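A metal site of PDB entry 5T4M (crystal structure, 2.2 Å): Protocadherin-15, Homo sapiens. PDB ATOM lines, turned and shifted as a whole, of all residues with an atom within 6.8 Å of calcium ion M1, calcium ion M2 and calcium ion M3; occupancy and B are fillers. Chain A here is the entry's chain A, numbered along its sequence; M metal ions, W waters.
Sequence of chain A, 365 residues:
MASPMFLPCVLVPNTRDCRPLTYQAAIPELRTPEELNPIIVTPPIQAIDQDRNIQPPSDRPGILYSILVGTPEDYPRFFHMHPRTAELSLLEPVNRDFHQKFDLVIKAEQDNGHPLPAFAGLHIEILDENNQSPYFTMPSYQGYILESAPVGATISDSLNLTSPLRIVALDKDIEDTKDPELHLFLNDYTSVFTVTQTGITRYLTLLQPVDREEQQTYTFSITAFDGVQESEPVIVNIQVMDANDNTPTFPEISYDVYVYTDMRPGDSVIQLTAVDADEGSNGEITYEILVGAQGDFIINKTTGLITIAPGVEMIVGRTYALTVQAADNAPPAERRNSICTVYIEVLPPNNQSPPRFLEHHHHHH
The side-chain amide nitrogen of Asn 246 sits close to the side-chain carboxylate of Glu 213, at 3.2 Å. The backbone NH of Arg 212 lies close to the side-chain carboxylate of Glu 147 (3.1 Å). The backbone NH of Glu 147 sits at hydrogen-bond distance from the backbone carbonyl oxygen of Met 241 (3.1 Å). The side-chain amide nitrogen of Asn 282 is in hydrogen-bond range of the side-chain carboxylate of Asp 242. The guanidinium group (NE) of Arg 212 sits close to the side-chain carboxylate (OD1) of Asp 242. The side-chain carboxylate (OD2) of Asp 242 sits at hydrogen-bond distance from the backbone NH (N) of Glu 279, 2.8 Å away. ND2 of Asn 244 lies within hydrogen-bond range of O of Glu 334, 2.7 Å away. The backbone NH of Arg 336 lies within hydrogen-bond range of the side-chain carboxylate of Asp 328 (2.9 Å).
Calcium ion M3 is bound by OD2 of Asp 276 (2.3 Å), O of Asn 246 (2.3 Å), OD1 of Asn 244 (2.4 Å), OD2 of Asp 278 (2.4 Å), O of Asn 282 (2.4 Å), OD1 of Asp 276 (2.5 Å) and OD2 of Asp 328 (2.6 Å).
Calcium ion M1 is bound by OE1 of Glu 213 (2.3 Å), water W1 (2.3 Å), OD1 of Asp 211 (2.3 Å), OE2 of Glu 147 (2.3 Å), OD2 of Asp 245 (2.3 Å), water W2 (2.5 Å) and OD1 of Asp 245 (2.7 Å).
The nearest printed residue that does not touch calcium ion M1 is Arg 212 (4.4 Å).
Calcium ion M2 is bound by OD1 of Asp 278 (2.3 Å), OD1 of Asp 242 (2.4 Å), OE1 of Glu 147 (2.4 Å), O of Ala 243 (2.4 Å), OD1 of Asp 245 (2.5 Å), OE2 of Glu 213 (2.5 Å) and OE1 of Glu 213 (2.5 Å).
The nearest printed residue that does not touch calcium ion M3 is Gly 283 (4.5 Å).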
ATOM      1  N   GLU A 147      -5.039 -15.487 -22.613  1.00  0.00           N
ATOM      2  CA  GLU A 147      -4.836 -15.879 -24.010  1.00  0.00           C
ATOM      3  C   GLU A 147      -5.919 -15.336 -24.945  1.00  0.00           C
ATOM      4  O   GLU A 147      -5.717 -15.263 -26.158  1.00  0.00           O
ATOM      5  CB  GLU A 147      -4.779 -17.405 -24.133  1.00  0.00           C
ATOM      6  CG  GLU A 147      -6.088 -18.134 -23.859  1.00  0.00           C
ATOM      7  CD  GLU A 147      -5.965 -19.633 -24.080  1.00  0.00           C
ATOM      8  OE1 GLU A 147      -6.391 -20.418 -23.210  1.00  0.00           O
ATOM      9  OE2 GLU A 147      -5.425 -20.032 -25.141  1.00  0.00           O
ATOM     10  N   VAL A 210      -1.815 -14.526 -28.429  1.00  0.00           N
ATOM     11  CA  VAL A 210      -1.091 -15.688 -27.936  1.00  0.00           C
ATOM     12  C   VAL A 210      -2.060 -16.815 -27.606  1.00  0.00           C
ATOM     13  O   VAL A 210      -3.211 -16.581 -27.247  1.00  0.00           O
ATOM     14  CB  VAL A 210      -0.240 -15.350 -26.684  1.00  0.00           C
ATOM     15  CG1 VAL A 210       0.959 -14.510 -27.082  1.00  0.00           C
ATOM     16  CG2 VAL A 210      -1.082 -14.640 -25.640  1.00  0.00           C
ATOM     17  N   ASP A 211      -1.578 -18.049 -27.734  1.00  0.00           N
ATOM     18  CA  ASP A 211      -2.392 -19.229 -27.516  1.00  0.00           C
ATOM     19  C   ASP A 211      -1.717 -20.123 -26.480  1.00  0.00           C
ATOM     20  O   ASP A 211      -0.672 -20.715 -26.741  1.00  0.00           O
ATOM     21  CB  ASP A 211      -2.597 -19.980 -28.835  1.00  0.00           C
ATOM     22  CG  ASP A 211      -3.399 -21.262 -28.691  1.00  0.00           C
ATOM     23  OD1 ASP A 211      -4.067 -21.452 -27.651  1.00  0.00           O
ATOM     24  OD2 ASP A 211      -3.370 -22.092 -29.622  1.00  0.00           O
ATOM     25  N   ARG A 212      -2.328 -20.212 -25.291  1.00  0.00           N
ATOM     26  CA  ARG A 212      -1.755 -20.982 -24.199  1.00  0.00           C
ATOM     27  C   ARG A 212      -1.485 -22.413 -24.602  1.00  0.00           C
ATOM     28  O   ARG A 212      -0.456 -22.988 -24.238  1.00  0.00           O
ATOM     29  CB  ARG A 212      -2.661 -20.973 -22.967  1.00  0.00           C
ATOM     30  CG  ARG A 212      -1.961 -21.491 -21.713  1.00  0.00           C
ATOM     31  CD  ARG A 212      -2.918 -22.101 -20.710  1.00  0.00           C
ATOM     32  NE  ARG A 212      -3.611 -23.257 -21.262  1.00  0.00           N
ATOM     33  CZ  ARG A 212      -3.145 -24.501 -21.241  1.00  0.00           C
ATOM     34  NH1 ARG A 212      -1.970 -24.762 -20.671  1.00  0.00           N
ATOM     35  NH2 ARG A 212      -3.856 -25.487 -21.776  1.00  0.00           N
ATOM     36  N   GLU A 213      -2.407 -22.989 -25.374  1.00  0.00           N
ATOM     37  CA  GLU A 213      -2.268 -24.375 -25.830  1.00  0.00           C
ATOM     38  C   GLU A 213      -1.063 -24.540 -26.768  1.00  0.00           C
ATOM     39  O   GLU A 213      -0.572 -25.649 -26.976  1.00  0.00           O
ATOM     40  CB  GLU A 213      -3.551 -24.854 -26.508  1.00  0.00           C
ATOM     41  CG  GLU A 213      -4.664 -25.280 -25.547  1.00  0.00           C
ATOM     42  CD  GLU A 213      -5.282 -24.121 -24.778  1.00  0.00           C
ATOM     43  OE1 GLU A 213      -5.707 -23.129 -25.408  1.00  0.00           O
ATOM     44  OE2 GLU A 213      -5.356 -24.198 -23.535  1.00  0.00           O
ATOM     45  N   GLU A 214      -0.601 -23.427 -27.345  1.00  0.00           N
ATOM     46  CA  GLU A 214       0.565 -23.423 -28.219  1.00  0.00           C
ATOM     47  C   GLU A 214       1.851 -23.163 -27.431  1.00  0.00           C
ATOM     48  O   GLU A 214       2.818 -23.892 -27.572  1.00  0.00           O
ATOM     49  CB  GLU A 214       0.383 -22.379 -29.320  1.00  0.00           C
ATOM     50  CG  GLU A 214       1.283 -22.558 -30.531  1.00  0.00           C
ATOM     51  CD  GLU A 214       0.934 -21.604 -31.657  1.00  0.00           C
ATOM     52  OE1 GLU A 214       0.654 -20.420 -31.380  1.00  0.00           O
ATOM     53  OE2 GLU A 214       0.936 -22.041 -32.829  1.00  0.00           O
ATOM     54  N   MET A 241      -2.355 -17.050 -19.511  1.00  0.00           N
ATOM     55  CA  MET A 241      -3.397 -17.680 -18.701  1.00  0.00           C
ATOM     56  C   MET A 241      -4.499 -18.314 -19.540  1.00  0.00           C
ATOM     57  O   MET A 241      -4.868 -17.797 -20.606  1.00  0.00           O
ATOM     58  CB  MET A 241      -3.983 -16.651 -17.726  1.00  0.00           C
ATOM     59  CG  MET A 241      -2.962 -16.129 -16.720  1.00  0.00           C
ATOM     60  SD  MET A 241      -3.609 -14.835 -15.648  1.00  0.00           S
ATOM     61  CE  MET A 241      -4.743 -15.761 -14.623  1.00  0.00           C
ATOM     62  N   ASP A 242      -5.017 -19.429 -19.058  1.00  0.00           N
ATOM     63  CA  ASP A 242      -5.967 -20.242 -19.818  1.00  0.00           C
ATOM     64  C   ASP A 242      -7.336 -19.602 -19.949  1.00  0.00           C
ATOM     65  O   ASP A 242      -7.898 -19.084 -18.983  1.00  0.00           O
ATOM     66  CB  ASP A 242      -6.106 -21.625 -19.168  1.00  0.00           C
ATOM     67  CG  ASP A 242      -6.887 -22.601 -20.034  1.00  0.00           C
ATOM     68  OD1 ASP A 242      -6.656 -22.643 -21.261  1.00  0.00           O
ATOM     69  OD2 ASP A 242      -7.740 -23.330 -19.483  1.00  0.00           O
ATOM     70  N   ALA A 243      -7.853 -19.611 -21.176  1.00  0.00           N
ATOM     71  CA  ALA A 243      -9.269 -19.375 -21.417  1.00  0.00           C
ATOM     72  C   ALA A 243      -9.888 -20.693 -21.833  1.00  0.00           C
ATOM     73  O   ALA A 243      -9.224 -21.526 -22.453  1.00  0.00           O
ATOM     74  CB  ALA A 243      -9.469 -18.319 -22.483  1.00  0.00           C
ATOM     75  N   ASN A 244     -11.155 -20.900 -21.496  1.00  0.00           N
ATOM     76  CA  ASN A 244     -11.839 -22.105 -21.959  1.00  0.00           C
ATOM     77  C   ASN A 244     -12.233 -21.944 -23.416  1.00  0.00           C
ATOM     78  O   ASN A 244     -13.393 -21.657 -23.728  1.00  0.00           O
ATOM     79  CB  ASN A 244     -13.080 -22.396 -21.100  1.00  0.00           C
ATOM     80  CG  ASN A 244     -13.594 -23.805 -21.308  1.00  0.00           C
ATOM     81  OD1 ASN A 244     -12.816 -24.749 -21.435  1.00  0.00           O
ATOM     82  ND2 ASN A 244     -14.913 -23.959 -21.372  1.00  0.00           N
ATOM     83  N   ASP A 245     -11.247 -22.108 -24.295  1.00  0.00           N
ATOM     84  CA  ASP A 245     -11.452 -21.924 -25.726  1.00  0.00           C
ATOM     85  C   ASP A 245     -11.233 -23.224 -26.486  1.00  0.00           C
ATOM     86  O   ASP A 245     -11.009 -23.217 -27.699  1.00  0.00           O
ATOM     87  CB  ASP A 245     -10.549 -20.789 -26.261  1.00  0.00           C
ATOM     88  CG  ASP A 245      -9.061 -21.169 -26.338  1.00  0.00           C
ATOM     89  OD1 ASP A 245      -8.565 -22.043 -25.591  1.00  0.00           O
ATOM     90  OD2 ASP A 245      -8.366 -20.540 -27.164  1.00  0.00           O
ATOM     91  N   ASN A 246     -11.306 -24.339 -25.767  1.00  0.00           N
ATOM     92  CA  ASN A 246     -11.339 -25.667 -26.379  1.00  0.00           C
ATOM     93  C   ASN A 246     -12.536 -26.495 -25.889  1.00  0.00           C
ATOM     94  O   ASN A 246     -12.842 -26.529 -24.707  1.00  0.00           O
ATOM     95  CB  ASN A 246     -10.046 -26.426 -26.095  1.00  0.00           C
ATOM     96  CG  ASN A 246      -8.892 -25.912 -26.921  1.00  0.00           C
ATOM     97  OD1 ASN A 246      -8.575 -26.470 -27.973  1.00  0.00           O
ATOM     98  ND2 ASN A 246      -8.263 -24.823 -26.468  1.00  0.00           N
ATOM     99  N   THR A 247     -13.190 -27.151 -26.840  1.00  0.00           N
ATOM    100  CA  THR A 247     -14.389 -27.934 -26.571  1.00  0.00           C
ATOM    101  C   THR A 247     -14.046 -29.417 -26.458  1.00  0.00           C
ATOM    102  O   THR A 247     -13.275 -29.933 -27.257  1.00  0.00           O
ATOM    103  CB  THR A 247     -15.440 -27.725 -27.688  1.00  0.00           C
ATOM    104  OG1 THR A 247     -15.896 -26.368 -27.673  1.00  0.00           O
ATOM    105  CG2 THR A 247     -16.635 -28.661 -27.533  1.00  0.00           C
ATOM    106  N   PRO A 248     -14.608 -30.106 -25.441  1.00  0.00           N
ATOM    107  CA  PRO A 248     -14.421 -31.555 -25.330  1.00  0.00           C
ATOM    108  C   PRO A 248     -14.823 -32.253 -26.627  1.00  0.00           C
ATOM    109  O   PRO A 248     -15.941 -32.062 -27.099  1.00  0.00           O
ATOM    110  CB  PRO A 248     -15.360 -31.949 -24.182  1.00  0.00           C
ATOM    111  CG  PRO A 248     -15.476 -30.713 -23.364  1.00  0.00           C
ATOM    112  CD  PRO A 248     -15.409 -29.560 -24.335  1.00  0.00           C
ATOM    113  N   ASP A 276      -9.915 -32.517 -24.370  1.00  0.00           N
ATOM    114  CA  ASP A 276      -9.999 -31.087 -24.100  1.00  0.00           C
ATOM    115  C   ASP A 276      -8.603 -30.589 -23.709  1.00  0.00           C
ATOM    116  O   ASP A 276      -8.025 -31.064 -22.734  1.00  0.00           O
ATOM    117  CB  ASP A 276     -11.020 -30.802 -22.995  1.00  0.00           C
ATOM    118  CG  ASP A 276     -11.454 -29.339 -22.949  1.00  0.00           C
ATOM    119  OD1 ASP A 276     -10.591 -28.436 -22.907  1.00  0.00           O
ATOM    120  OD2 ASP A 276     -12.680 -29.103 -22.953  1.00  0.00           O
ATOM    121  N   ALA A 277      -8.058 -29.651 -24.480  1.00  0.00           N
ATOM    122  CA  ALA A 277      -6.668 -29.222 -24.316  1.00  0.00           C
ATOM    123  C   ALA A 277      -6.508 -28.096 -23.297  1.00  0.00           C
ATOM    124  O   ALA A 277      -5.388 -27.686 -23.007  1.00  0.00           O
ATOM    125  CB  ALA A 277      -6.102 -28.794 -25.663  1.00  0.00           C
ATOM    126  N   ASP A 278      -7.614 -27.601 -22.764  1.00  0.00           N
ATOM    127  CA  ASP A 278      -7.564 -26.494 -21.819  1.00  0.00           C
ATOM    128  C   ASP A 278      -6.959 -26.931 -20.478  1.00  0.00           C
ATOM    129  O   ASP A 278      -6.733 -28.125 -20.247  1.00  0.00           O
ATOM    130  CB  ASP A 278      -8.962 -25.910 -21.605  1.00  0.00           C
ATOM    131  CG  ASP A 278      -9.487 -25.216 -22.839  1.00  0.00           C
ATOM    132  OD1 ASP A 278      -8.704 -24.539 -23.533  1.00  0.00           O
ATOM    133  OD2 ASP A 278     -10.695 -25.358 -23.133  1.00  0.00           O
ATOM    134  N   GLU A 279      -6.716 -25.965 -19.607  1.00  0.00           N
ATOM    135  CA  GLU A 279      -5.997 -26.218 -18.362  1.00  0.00           C
ATOM    136  C   GLU A 279      -6.949 -26.442 -17.188  1.00  0.00           C
ATOM    137  O   GLU A 279      -7.985 -25.798 -17.085  1.00  0.00           O
ATOM    138  CB  GLU A 279      -5.060 -25.047 -18.059  1.00  0.00           C
ATOM    139  CG  GLU A 279      -4.031 -25.307 -16.985  1.00  0.00           C
ATOM    140  CD  GLU A 279      -3.095 -24.137 -16.763  1.00  0.00           C
ATOM    141  OE1 GLU A 279      -1.905 -24.363 -16.471  1.00  0.00           O
ATOM    142  OE2 GLU A 279      -3.552 -22.971 -16.891  1.00  0.00           O
ATOM    143  N   SER A 281      -9.672 -27.325 -14.621  1.00  0.00           N
ATOM    144  CA  SER A 281     -11.092 -27.635 -14.713  1.00  0.00           C
ATOM    145  C   SER A 281     -11.659 -27.267 -16.087  1.00  0.00           C
ATOM    146  O   SER A 281     -12.700 -27.800 -16.489  1.00  0.00           O
ATOM    147  CB  SER A 281     -11.866 -26.905 -13.606  1.00  0.00           C
ATOM    148  OG  SER A 281     -11.861 -25.503 -13.806  1.00  0.00           O
ATOM    149  N   ASN A 282     -10.978 -26.375 -16.797  1.00  0.00           N
ATOM    150  CA  ASN A 282     -11.361 -26.035 -18.162  1.00  0.00           C
ATOM    151  C   ASN A 282     -11.140 -27.209 -19.114  1.00  0.00           C
ATOM    152  O   ASN A 282     -11.767 -27.307 -20.170  1.00  0.00           O
ATOM    153  CB  ASN A 282     -10.601 -24.805 -18.663  1.00  0.00           C
ATOM    154  CG  ASN A 282     -11.089 -23.516 -18.034  1.00  0.00           C
ATOM    155  OD1 ASN A 282     -12.207 -23.434 -17.539  1.00  0.00           O
ATOM    156  ND2 ASN A 282     -10.245 -22.483 -18.078  1.00  0.00           N
ATOM    157  N   GLY A 283     -10.235 -28.107 -18.725  1.00  0.00           N
ATOM    158  CA  GLY A 283      -9.961 -29.299 -19.498  1.00  0.00           C
ATOM    159  C   GLY A 283     -10.540 -30.560 -18.871  1.00  0.00           C
ATOM    160  O   GLY A 283     -10.466 -31.646 -19.460  1.00  0.00           O
ATOM    161  N   GLU A 284     -11.098 -30.420 -17.675  1.00  0.00           N
ATOM    162  CA  GLU A 284     -11.673 -31.546 -16.950  1.00  0.00           C
ATOM    163  C   GLU A 284     -13.011 -31.975 -17.551  1.00  0.00           C
ATOM    164  O   GLU A 284     -13.973 -31.209 -17.543  1.00  0.00           O
ATOM    165  CB  GLU A 284     -11.855 -31.179 -15.472  1.00  0.00           C
ATOM    166  CG  GLU A 284     -12.376 -32.298 -14.593  1.00  0.00           C
ATOM    167  CD  GLU A 284     -12.608 -31.856 -13.158  1.00  0.00           C
ATOM    168  OE1 GLU A 284     -12.238 -30.703 -12.821  1.00  0.00           O
ATOM    169  OE2 GLU A 284     -13.152 -32.650 -12.369  1.00  0.00           O
ATOM    170  N   ASP A 328     -16.865 -29.935 -20.279  1.00  0.00           N
ATOM    171  CA  ASP A 328     -15.777 -29.561 -19.378  1.00  0.00           C
ATOM    172  C   ASP A 328     -16.332 -28.941 -18.106  1.00  0.00           C
ATOM    173  O   ASP A 328     -17.507 -28.564 -18.052  1.00  0.00           O
ATOM    174  CB  ASP A 328     -14.771 -28.612 -20.061  1.00  0.00           C
ATOM    175  CG  ASP A 328     -15.421 -27.394 -20.704  1.00  0.00           C
ATOM    176  OD1 ASP A 328     -16.462 -26.910 -20.210  1.00  0.00           O
ATOM    177  OD2 ASP A 328     -14.862 -26.913 -21.713  1.00  0.00           O
ATOM    178  N   ASN A 329     -15.501 -28.852 -17.077  1.00  0.00           N
ATOM    179  CA  ASN A 329     -15.946 -28.352 -15.785  1.00  0.00           C
ATOM    180  C   ASN A 329     -15.557 -26.895 -15.540  1.00  0.00           C
ATOM    181  O   ASN A 329     -15.168 -26.520 -14.434  1.00  0.00           O
ATOM    182  CB  ASN A 329     -15.402 -29.236 -14.660  1.00  0.00           C
ATOM    183  CG  ASN A 329     -16.268 -30.461 -14.434  1.00  0.00           C
ATOM    184  OD1 ASN A 329     -16.053 -31.509 -15.049  1.00  0.00           O
ATOM    185  ND2 ASN A 329     -17.253 -30.338 -13.554  1.00  0.00           N
ATOM    186  N   ALA A 330     -15.668 -26.098 -16.592  1.00  0.00           N
ATOM    187  CA  ALA A 330     -15.592 -24.655 -16.452  1.00  0.00           C
ATOM    188  C   ALA A 330     -16.897 -24.189 -15.824  1.00  0.00           C
ATOM    189  O   ALA A 330     -17.877 -24.918 -15.826  1.00  0.00           O
ATOM    190  CB  ALA A 330     -15.371 -24.000 -17.812  1.00  0.00           C
ATOM    191  N   GLU A 334     -19.127 -20.420 -19.104  1.00  0.00           N
ATOM    192  CA  GLU A 334     -18.076 -20.649 -20.089  1.00  0.00           C
ATOM    193  C   GLU A 334     -17.967 -22.107 -20.512  1.00  0.00           C
ATOM    194  O   GLU A 334     -17.102 -22.466 -21.313  1.00  0.00           O
ATOM    195  CB  GLU A 334     -16.724 -20.179 -19.543  1.00  0.00           C
ATOM    196  CG  GLU A 334     -16.668 -18.706 -19.160  1.00  0.00           C
ATOM    197  CD  GLU A 334     -16.646 -18.519 -17.657  1.00  0.00           C
ATOM    198  OE1 GLU A 334     -17.724 -18.599 -17.018  1.00  0.00           O
ATOM    199  OE2 GLU A 334     -15.552 -18.290 -17.102  1.00  0.00           O
ATOM    200  N   ARG A 336     -18.217 -25.716 -22.141  1.00  0.00           N
ATOM    201  CA  ARG A 336     -18.336 -26.212 -23.506  1.00  0.00           C
ATOM    202  C   ARG A 336     -18.625 -27.714 -23.507  1.00  0.00           C
ATOM    203  O   ARG A 336     -18.169 -28.437 -22.626  1.00  0.00           O
ATOM    204  CB  ARG A 336     -17.065 -25.932 -24.301  1.00  0.00           C
ATOM    205  CG  ARG A 336     -16.861 -24.482 -24.666  1.00  0.00           C
ATOM    206  CD  ARG A 336     -15.470 -24.250 -25.228  1.00  0.00           C
ATOM    207  NE  ARG A 336     -15.323 -22.874 -25.708  1.00  0.00           N
ATOM    208  CZ  ARG A 336     -15.383 -22.535 -26.997  1.00  0.00           C
ATOM    209  NH1 ARG A 336     -15.558 -23.469 -27.920  1.00  0.00           N
ATOM    210  NH2 ARG A 336     -15.249 -21.259 -27.350  1.00  0.00           N
HETATM  211 CA    CA M   1      -6.225 -21.418 -26.819  1.00  0.00          CA
HETATM  212 CA    CA M   2      -7.338 -22.638 -23.519  1.00  0.00          CA
HETATM  213 CA    CA M   3     -12.405 -26.857 -22.422  1.00  0.00          CA
HETATM  214  O   HOH W   1      -5.968 -19.730 -28.339  1.00  0.00           O
HETATM  215  O   HOH W   2      -6.956 -23.136 -28.434  1.00  0.00           O
